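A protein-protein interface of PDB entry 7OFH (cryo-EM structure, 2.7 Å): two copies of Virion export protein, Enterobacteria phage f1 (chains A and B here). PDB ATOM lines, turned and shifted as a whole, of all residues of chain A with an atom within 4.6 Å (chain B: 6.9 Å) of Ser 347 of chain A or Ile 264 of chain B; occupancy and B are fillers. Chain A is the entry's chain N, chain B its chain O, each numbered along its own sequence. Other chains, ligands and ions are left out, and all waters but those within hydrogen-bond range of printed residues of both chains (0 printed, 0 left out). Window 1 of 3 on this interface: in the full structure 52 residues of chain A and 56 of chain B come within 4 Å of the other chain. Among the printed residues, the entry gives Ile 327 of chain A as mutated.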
ATOM      1  N   ILE A 327      16.860  34.769   5.891  1.00  0.00           N
ATOM      2  CA  ILE A 327      17.876  35.689   5.400  1.00  0.00           C
ATOM      3  C   ILE A 327      18.886  34.874   4.608  1.00  0.00           C
ATOM      4  O   ILE A 327      19.484  33.969   5.154  1.00  0.00           O
ATOM      5  CB  ILE A 327      18.519  36.453   6.575  1.00  0.00           C
ATOM      6  CG1 ILE A 327      17.578  37.499   7.152  1.00  0.00           C
ATOM      7  CG2 ILE A 327      19.813  37.122   6.190  1.00  0.00           C
ATOM      8  CD1 ILE A 327      18.113  38.210   8.364  1.00  0.00           C
ATOM      9  N   LYS A 328      19.090  35.177   3.326  1.00  0.00           N
ATOM     10  CA  LYS A 328      20.095  34.505   2.512  1.00  0.00           C
ATOM     11  C   LYS A 328      21.133  35.515   2.018  1.00  0.00           C
ATOM     12  O   LYS A 328      20.764  36.488   1.383  1.00  0.00           O
ATOM     13  CB  LYS A 328      19.462  33.928   1.241  1.00  0.00           C
ATOM     14  CG  LYS A 328      18.648  32.662   1.420  1.00  0.00           C
ATOM     15  CD  LYS A 328      18.299  32.010   0.111  1.00  0.00           C
ATOM     16  CE  LYS A 328      17.107  32.649  -0.571  1.00  0.00           C
ATOM     17  NZ  LYS A 328      16.084  33.097   0.407  1.00  0.00           N
ATOM     18  N   GLN A 345      27.101  30.144  -0.267  1.00  0.00           N
ATOM     19  CA  GLN A 345      25.811  30.256   0.394  1.00  0.00           C
ATOM     20  C   GLN A 345      25.996  30.679   1.846  1.00  0.00           C
ATOM     21  O   GLN A 345      27.017  30.416   2.477  1.00  0.00           O
ATOM     22  CB  GLN A 345      25.046  28.945   0.182  1.00  0.00           C
ATOM     23  CG  GLN A 345      24.626  28.207   1.441  1.00  0.00           C
ATOM     24  CD  GLN A 345      23.137  28.318   1.626  1.00  0.00           C
ATOM     25  OE1 GLN A 345      22.511  27.448   2.232  1.00  0.00           O
ATOM     26  NE2 GLN A 345      22.555  29.379   1.075  1.00  0.00           N
ATOM     27  N   ARG A 346      24.989  31.367   2.372  1.00  0.00           N
ATOM     28  CA  ARG A 346      24.863  31.672   3.785  1.00  0.00           C
ATOM     29  C   ARG A 346      23.388  31.928   4.037  1.00  0.00           C
ATOM     30  O   ARG A 346      22.876  32.933   3.558  1.00  0.00           O
ATOM     31  CB  ARG A 346      25.618  32.956   4.130  1.00  0.00           C
ATOM     32  CG  ARG A 346      26.916  32.756   4.888  1.00  0.00           C
ATOM     33  CD  ARG A 346      27.740  34.026   4.948  1.00  0.00           C
ATOM     34  NE  ARG A 346      27.552  34.768   3.722  1.00  0.00           N
ATOM     35  CZ  ARG A 346      28.157  35.905   3.417  1.00  0.00           C
ATOM     36  NH1 ARG A 346      27.894  36.499   2.263  1.00  0.00           N
ATOM     37  NH2 ARG A 346      29.025  36.446   4.252  1.00  0.00           N
ATOM     38  N   SER A 347      22.703  31.050   4.784  1.00  0.00           N
ATOM     39  CA  SER A 347      21.272  31.209   5.009  1.00  0.00           C
ATOM     40  C   SER A 347      20.857  30.849   6.433  1.00  0.00           C
ATOM     41  O   SER A 347      21.403  29.925   7.024  1.00  0.00           O
ATOM     42  CB  SER A 347      20.517  30.382   4.017  1.00  0.00           C
ATOM     43  OG  SER A 347      21.082  29.073   3.932  1.00  0.00           O
ATOM     44  N   ILE A 348      19.886  31.591   6.969  1.00  0.00           N
ATOM     45  CA  ILE A 348      19.192  31.245   8.195  1.00  0.00           C
ATOM     46  C   ILE A 348      17.713  31.199   7.843  1.00  0.00           C
ATOM     47  O   ILE A 348      17.211  32.073   7.144  1.00  0.00           O
ATOM     48  CB  ILE A 348      19.484  32.283   9.294  1.00  0.00           C
ATOM     49  CG1 ILE A 348      20.903  32.167   9.826  1.00  0.00           C
ATOM     50  CG2 ILE A 348      18.523  32.197  10.472  1.00  0.00           C
ATOM     51  CD1 ILE A 348      21.072  32.927  11.131  1.00  0.00           C
ATOM     52  N   ALA A 349      16.994  30.191   8.324  1.00  0.00           N
ATOM     53  CA  ALA A 349      15.551  30.282   8.237  1.00  0.00           C
ATOM     54  C   ALA A 349      14.970  29.816   9.549  1.00  0.00           C
ATOM     55  O   ALA A 349      15.234  28.703   9.962  1.00  0.00           O
ATOM     56  CB  ALA A 349      15.045  29.436   7.110  1.00  0.00           C
ATOM     57  N   GLY A 363      20.983  33.889  14.719  1.00  0.00           N
ATOM     58  CA  GLY A 363      21.860  32.753  14.466  1.00  0.00           C
ATOM     59  C   GLY A 363      23.309  33.162  14.214  1.00  0.00           C
ATOM     60  O   GLY A 363      23.694  34.258  14.587  1.00  0.00           O
ATOM     61  N   GLY A 364      24.137  32.273  13.655  1.00  0.00           N
ATOM     62  CA  GLY A 364      25.525  32.628  13.387  1.00  0.00           C
ATOM     63  C   GLY A 364      26.398  31.403  13.145  1.00  0.00           C
ATOM     64  O   GLY A 364      25.895  30.288  13.266  1.00  0.00           O
ATOM     65  N   PRO B 252      28.380  26.400  14.851  1.00  0.00           N
ATOM     66  CA  PRO B 252      27.115  26.918  14.347  1.00  0.00           C
ATOM     67  C   PRO B 252      26.119  27.257  15.448  1.00  0.00           C
ATOM     68  O   PRO B 252      26.176  26.666  16.515  1.00  0.00           O
ATOM     69  CB  PRO B 252      26.587  25.769  13.490  1.00  0.00           C
ATOM     70  CG  PRO B 252      27.168  24.560  14.126  1.00  0.00           C
ATOM     71  CD  PRO B 252      28.555  24.982  14.540  1.00  0.00           C
ATOM     72  N   ARG B 253      25.228  28.231  15.197  1.00  0.00           N
ATOM     73  CA  ARG B 253      24.201  28.646  16.149  1.00  0.00           C
ATOM     74  C   ARG B 253      22.906  29.058  15.444  1.00  0.00           C
ATOM     75  O   ARG B 253      22.941  29.537  14.309  1.00  0.00           O
ATOM     76  CB  ARG B 253      24.708  29.824  16.965  1.00  0.00           C
ATOM     77  CG  ARG B 253      25.728  29.408  18.000  1.00  0.00           C
ATOM     78  CD  ARG B 253      26.054  30.524  18.963  1.00  0.00           C
ATOM     79  NE  ARG B 253      26.576  31.724  18.360  1.00  0.00           N
ATOM     80  CZ  ARG B 253      27.074  32.739  19.057  1.00  0.00           C
ATOM     81  NH1 ARG B 253      27.110  32.683  20.379  1.00  0.00           N
ATOM     82  NH2 ARG B 253      27.542  33.809  18.431  1.00  0.00           N
ATOM     83  N   ILE B 254      21.770  28.841  16.119  1.00  0.00           N
ATOM     84  CA  ILE B 254      20.455  29.125  15.576  1.00  0.00           C
ATOM     85  C   ILE B 254      19.482  29.309  16.727  1.00  0.00           C
ATOM     86  O   ILE B 254      19.440  28.485  17.623  1.00  0.00           O
ATOM     87  CB  ILE B 254      19.990  28.007  14.626  1.00  0.00           C
ATOM     88  CG1 ILE B 254      18.693  28.335  13.903  1.00  0.00           C
ATOM     89  CG2 ILE B 254      19.858  26.673  15.338  1.00  0.00           C
ATOM     90  CD1 ILE B 254      18.897  29.277  12.750  1.00  0.00           C
ATOM     91  N   GLY B 262      14.264  25.253  12.503  1.00  0.00           N
ATOM     92  CA  GLY B 262      15.184  26.314  12.163  1.00  0.00           C
ATOM     93  C   GLY B 262      16.410  25.694  11.530  1.00  0.00           C
ATOM     94  O   GLY B 262      16.811  24.621  11.941  1.00  0.00           O
ATOM     95  N   SER B 263      17.006  26.379  10.559  1.00  0.00           N
ATOM     96  CA  SER B 263      18.214  25.843   9.972  1.00  0.00           C
ATOM     97  C   SER B 263      19.198  26.954   9.656  1.00  0.00           C
ATOM     98  O   SER B 263      18.806  28.056   9.302  1.00  0.00           O
ATOM     99  CB  SER B 263      17.877  25.079   8.743  1.00  0.00           C
ATOM    100  OG  SER B 263      17.153  25.910   7.838  1.00  0.00           O
ATOM    101  N   ILE B 264      20.485  26.639   9.798  1.00  0.00           N
ATOM    102  CA  ILE B 264      21.555  27.528   9.395  1.00  0.00           C
ATOM    103  C   ILE B 264      22.448  26.752   8.436  1.00  0.00           C
ATOM    104  O   ILE B 264      22.782  25.607   8.683  1.00  0.00           O
ATOM    105  CB  ILE B 264      22.305  28.061  10.633  1.00  0.00           C
ATOM    106  CG1 ILE B 264      23.348  29.114  10.273  1.00  0.00           C
ATOM    107  CG2 ILE B 264      22.920  26.950  11.467  1.00  0.00           C
ATOM    108  CD1 ILE B 264      23.535  30.153  11.337  1.00  0.00           C
ATOM    109  N   SER B 265      22.811  27.376   7.323  1.00  0.00           N
ATOM    110  CA  SER B 265      23.628  26.719   6.325  1.00  0.00           C
ATOM    111  C   SER B 265      24.632  27.720   5.778  1.00  0.00           C
ATOM    112  O   SER B 265      24.240  28.750   5.241  1.00  0.00           O
ATOM    113  CB  SER B 265      22.747  26.201   5.221  1.00  0.00           C
ATOM    114  OG  SER B 265      23.367  25.110   4.552  1.00  0.00           O
ATOM    115  N   VAL B 266      25.919  27.420   5.932  1.00  0.00           N
ATOM    116  CA  VAL B 266      26.962  28.287   5.425  1.00  0.00           C
ATOM    117  C   VAL B 266      27.915  27.397   4.659  1.00  0.00           C
ATOM    118  O   VAL B 266      28.464  26.455   5.222  1.00  0.00           O
ATOM    119  CB  VAL B 266      27.725  28.985   6.562  1.00  0.00           C
ATOM    120  CG1 VAL B 266      28.993  29.646   6.062  1.00  0.00           C
ATOM    121  CG2 VAL B 266      26.875  30.002   7.303  1.00  0.00           C
ATOM    122  N   GLY B 267      28.111  27.707   3.385  1.00  0.00           N
ATOM    123  CA  GLY B 267      29.007  26.907   2.588  1.00  0.00           C
ATOM    124  C   GLY B 267      28.930  27.287   1.124  1.00  0.00           C
ATOM    125  O   GLY B 267      29.125  28.439   0.762  1.00  0.00           O
ATOM    126  N   ASN B 295      23.533  21.980  -1.085  1.00  0.00           N
ATOM    127  CA  ASN B 295      24.413  22.752  -0.241  1.00  0.00           C
ATOM    128  C   ASN B 295      25.519  21.849   0.265  1.00  0.00           C
ATOM    129  O   ASN B 295      25.271  20.718   0.669  1.00  0.00           O
ATOM    130  CB  ASN B 295      23.650  23.325   0.941  1.00  0.00           C
ATOM    131  CG  ASN B 295      22.848  24.545   0.557  1.00  0.00           C
ATOM    132  OD1 ASN B 295      23.204  25.257  -0.380  1.00  0.00           O
ATOM    133  ND2 ASN B 295      21.785  24.815   1.294  1.00  0.00           N
ATOM    134  N   ILE B 298      28.843  23.695   6.235  1.00  0.00           N
ATOM    135  CA  ILE B 298      28.301  23.463   7.564  1.00  0.00           C
ATOM    136  C   ILE B 298      26.819  23.784   7.520  1.00  0.00           C
ATOM    137  O   ILE B 298      26.433  24.863   7.075  1.00  0.00           O
ATOM    138  CB  ILE B 298      28.976  24.347   8.627  1.00  0.00           C
ATOM    139  CG1 ILE B 298      30.499  24.322   8.590  1.00  0.00           C
ATOM    140  CG2 ILE B 298      28.494  23.986  10.007  1.00  0.00           C
ATOM    141  CD1 ILE B 298      31.082  22.982   8.946  1.00  0.00           C
ATOM    142  N   SER B 299      25.995  22.876   8.047  1.00  0.00           N
ATOM    143  CA  SER B 299      24.583  23.153   8.237  1.00  0.00           C
ATOM    144  C   SER B 299      24.093  22.494   9.513  1.00  0.00           C
ATOM    145  O   SER B 299      24.654  21.496   9.938  1.00  0.00           O
ATOM    146  CB  SER B 299      23.780  22.702   7.068  1.00  0.00           C
ATOM    147  OG  SER B 299      24.061  21.344   6.751  1.00  0.00           O
ATOM    148  N   MET B 300      23.062  23.074  10.129  1.00  0.00           N
ATOM    149  CA  MET B 300      22.471  22.496  11.305  1.00  0.00           C
ATOM    150  C   MET B 300      20.972  22.739  11.237  1.00  0.00           C
ATOM    151  O   MET B 300      20.524  23.873  11.263  1.00  0.00           O
ATOM    152  CB  MET B 300      23.085  23.181  12.516  1.00  0.00           C
ATOM    153  CG  MET B 300      22.581  22.693  13.818  1.00  0.00           C
ATOM    154  SD  MET B 300      23.584  23.371  15.116  1.00  0.00           S
ATOM    155  CE  MET B 300      22.785  24.955  15.389  1.00  0.00           C
ATOM    156  N   SER B 301      20.186  21.679  11.102  1.00  0.00           N
ATOM    157  CA  SER B 301      18.748  21.801  11.124  1.00  0.00           C
ATOM    158  C   SER B 301      18.277  21.339  12.477  1.00  0.00           C
ATOM    159  O   SER B 301      18.739  20.330  12.975  1.00  0.00           O
ATOM    160  CB  SER B 301      18.131  20.938  10.088  1.00  0.00           C
ATOM    161  OG  SER B 301      18.611  21.271   8.787  1.00  0.00           O
ATOM    162  N   VAL B 302      17.384  22.096  13.092  1.00  0.00           N
ATOM    163  CA  VAL B 302      16.943  21.735  14.418  1.00  0.00           C
ATOM    164  C   VAL B 302      15.434  21.718  14.430  1.00  0.00           C
ATOM    165  O   VAL B 302      14.804  22.361  13.613  1.00  0.00           O
ATOM    166  CB  VAL B 302      17.469  22.694  15.481  1.00  0.00           C
ATOM    167  CG1 VAL B 302      18.976  22.801  15.455  1.00  0.00           C
ATOM    168  CG2 VAL B 302      16.853  24.062  15.311  1.00  0.00           C
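Arg 346 of chain A touches Ser 265 of chain B. Ser 263 of chain B touches Ser 347 of chain A. Ser 347 of chain A touches Ile 264 of chain B (O to CA, 3.4 Å). CG2 of Ile 348 of chain A touches CD1 of Ile 254 of chain B, at 3.7 Å. Ile 348 of chain A touches Ser 263 of chain B. Ile 348 of chain A touches Ile 264 of chain B. Ala 349 of chain A touches Gly 262 of chain B (O to CA, 3.2 Å). Arg 253 of chain B touches Gly 363 of chain A. O of Gly 364 of chain A touches C of Pro 252 of chain B (3.7 Å). Ile 264 of chain B touches Gly 364 of chain A.
OE1 of Gln 345 of chain A is in hydrogen-bond range of ND2 of Asn 295 of chain B, at 2.9 Å. The side-chain amide oxygen (OE1) of Gln 345 of chain A sits close to the side-chain hydroxyl (OG) of Ser 265 of chain B (3.4 Å). N of Arg 253 of chain B sits at hydrogen-bond distance from O of Gly 364 of chain A (2.9 Å). N of Gln 345 of chain A is in hydrogen-bond range of O of Gly 267 of chain B, 2.8 Å away. N of Ala 349 of chain A lies within hydrogen-bond range of O of Ser 263 of chain B (3.0 Å). The backbone carbonyl oxygen (O) of Ser 265 of chain B sits at hydrogen-bond distance from the backbone NH (N) of Ser 347 of chain A (2.8 Å).
No position is printed for both chains. Of the 18 pairs that touch across the chains among the printed residues, none has its exchanged pair printed and touching as well.
The side-chain amide oxygen (OE1) of Gln 345 of chain A sits at hydrogen-bond distance from the side-chain hydroxyl (OG) of Ser 347 of chain A (2.8 Å). The backbone carbonyl oxygen of Ile 348 of chain A sits at hydrogen-bond distance from the backbone NH of Ile 327 of chain A, 3.0 Å away. N of Val 266 of chain B sits at hydrogen-bond distance from O of Ile 298 of chain B (2.8 Å). O of Gly 262 of chain B sits at hydrogen-bond distance from N of Val 302 of chain B (2.8 Å). The backbone carbonyl oxygen (O) of Ile 264 of chain B sits at hydrogen-bond distance from the backbone NH (N) of Met 300 of chain B (2.9 Å).
Ser 347 of chain A touches just these residues of chain B: Ser 263 (3.9 Å), Ile 264 (3.4 Å) and Ser 265 (2.8 Å). Printed residues of chain A within 4 Å of Pro 252 of chain B: Gly 364. Printed residues of chain A within 4 Å of Ile 254 of chain B: Ile 348 (3.7 Å). Printed residues of chain A within 4 Å of Ser 263 of chain B: Ser 347, Ile 348 and Ala 349. Printed residues of chain A within 4 Å of Ser 265 of chain B: Gln 345, Arg 346 and Ser 347. Ile 298 of chain B touches none of the printed residues of chain A. The nearest residue of chain B that does not touch Ser 347 of chain A is Val 266 of chain B (5.0 Å). The nearest printed residue of chain A that does not touch Ile 254 of chain B is Gly 363 of chain A (4.05 Å).
Of the 9 printed residues of chain A, 7 touch a printed residue of chain B. Hydrophobic or aromatic side chains of chain B that line the printed part of chain A: Ile 254, Ile 264 and Val 266.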
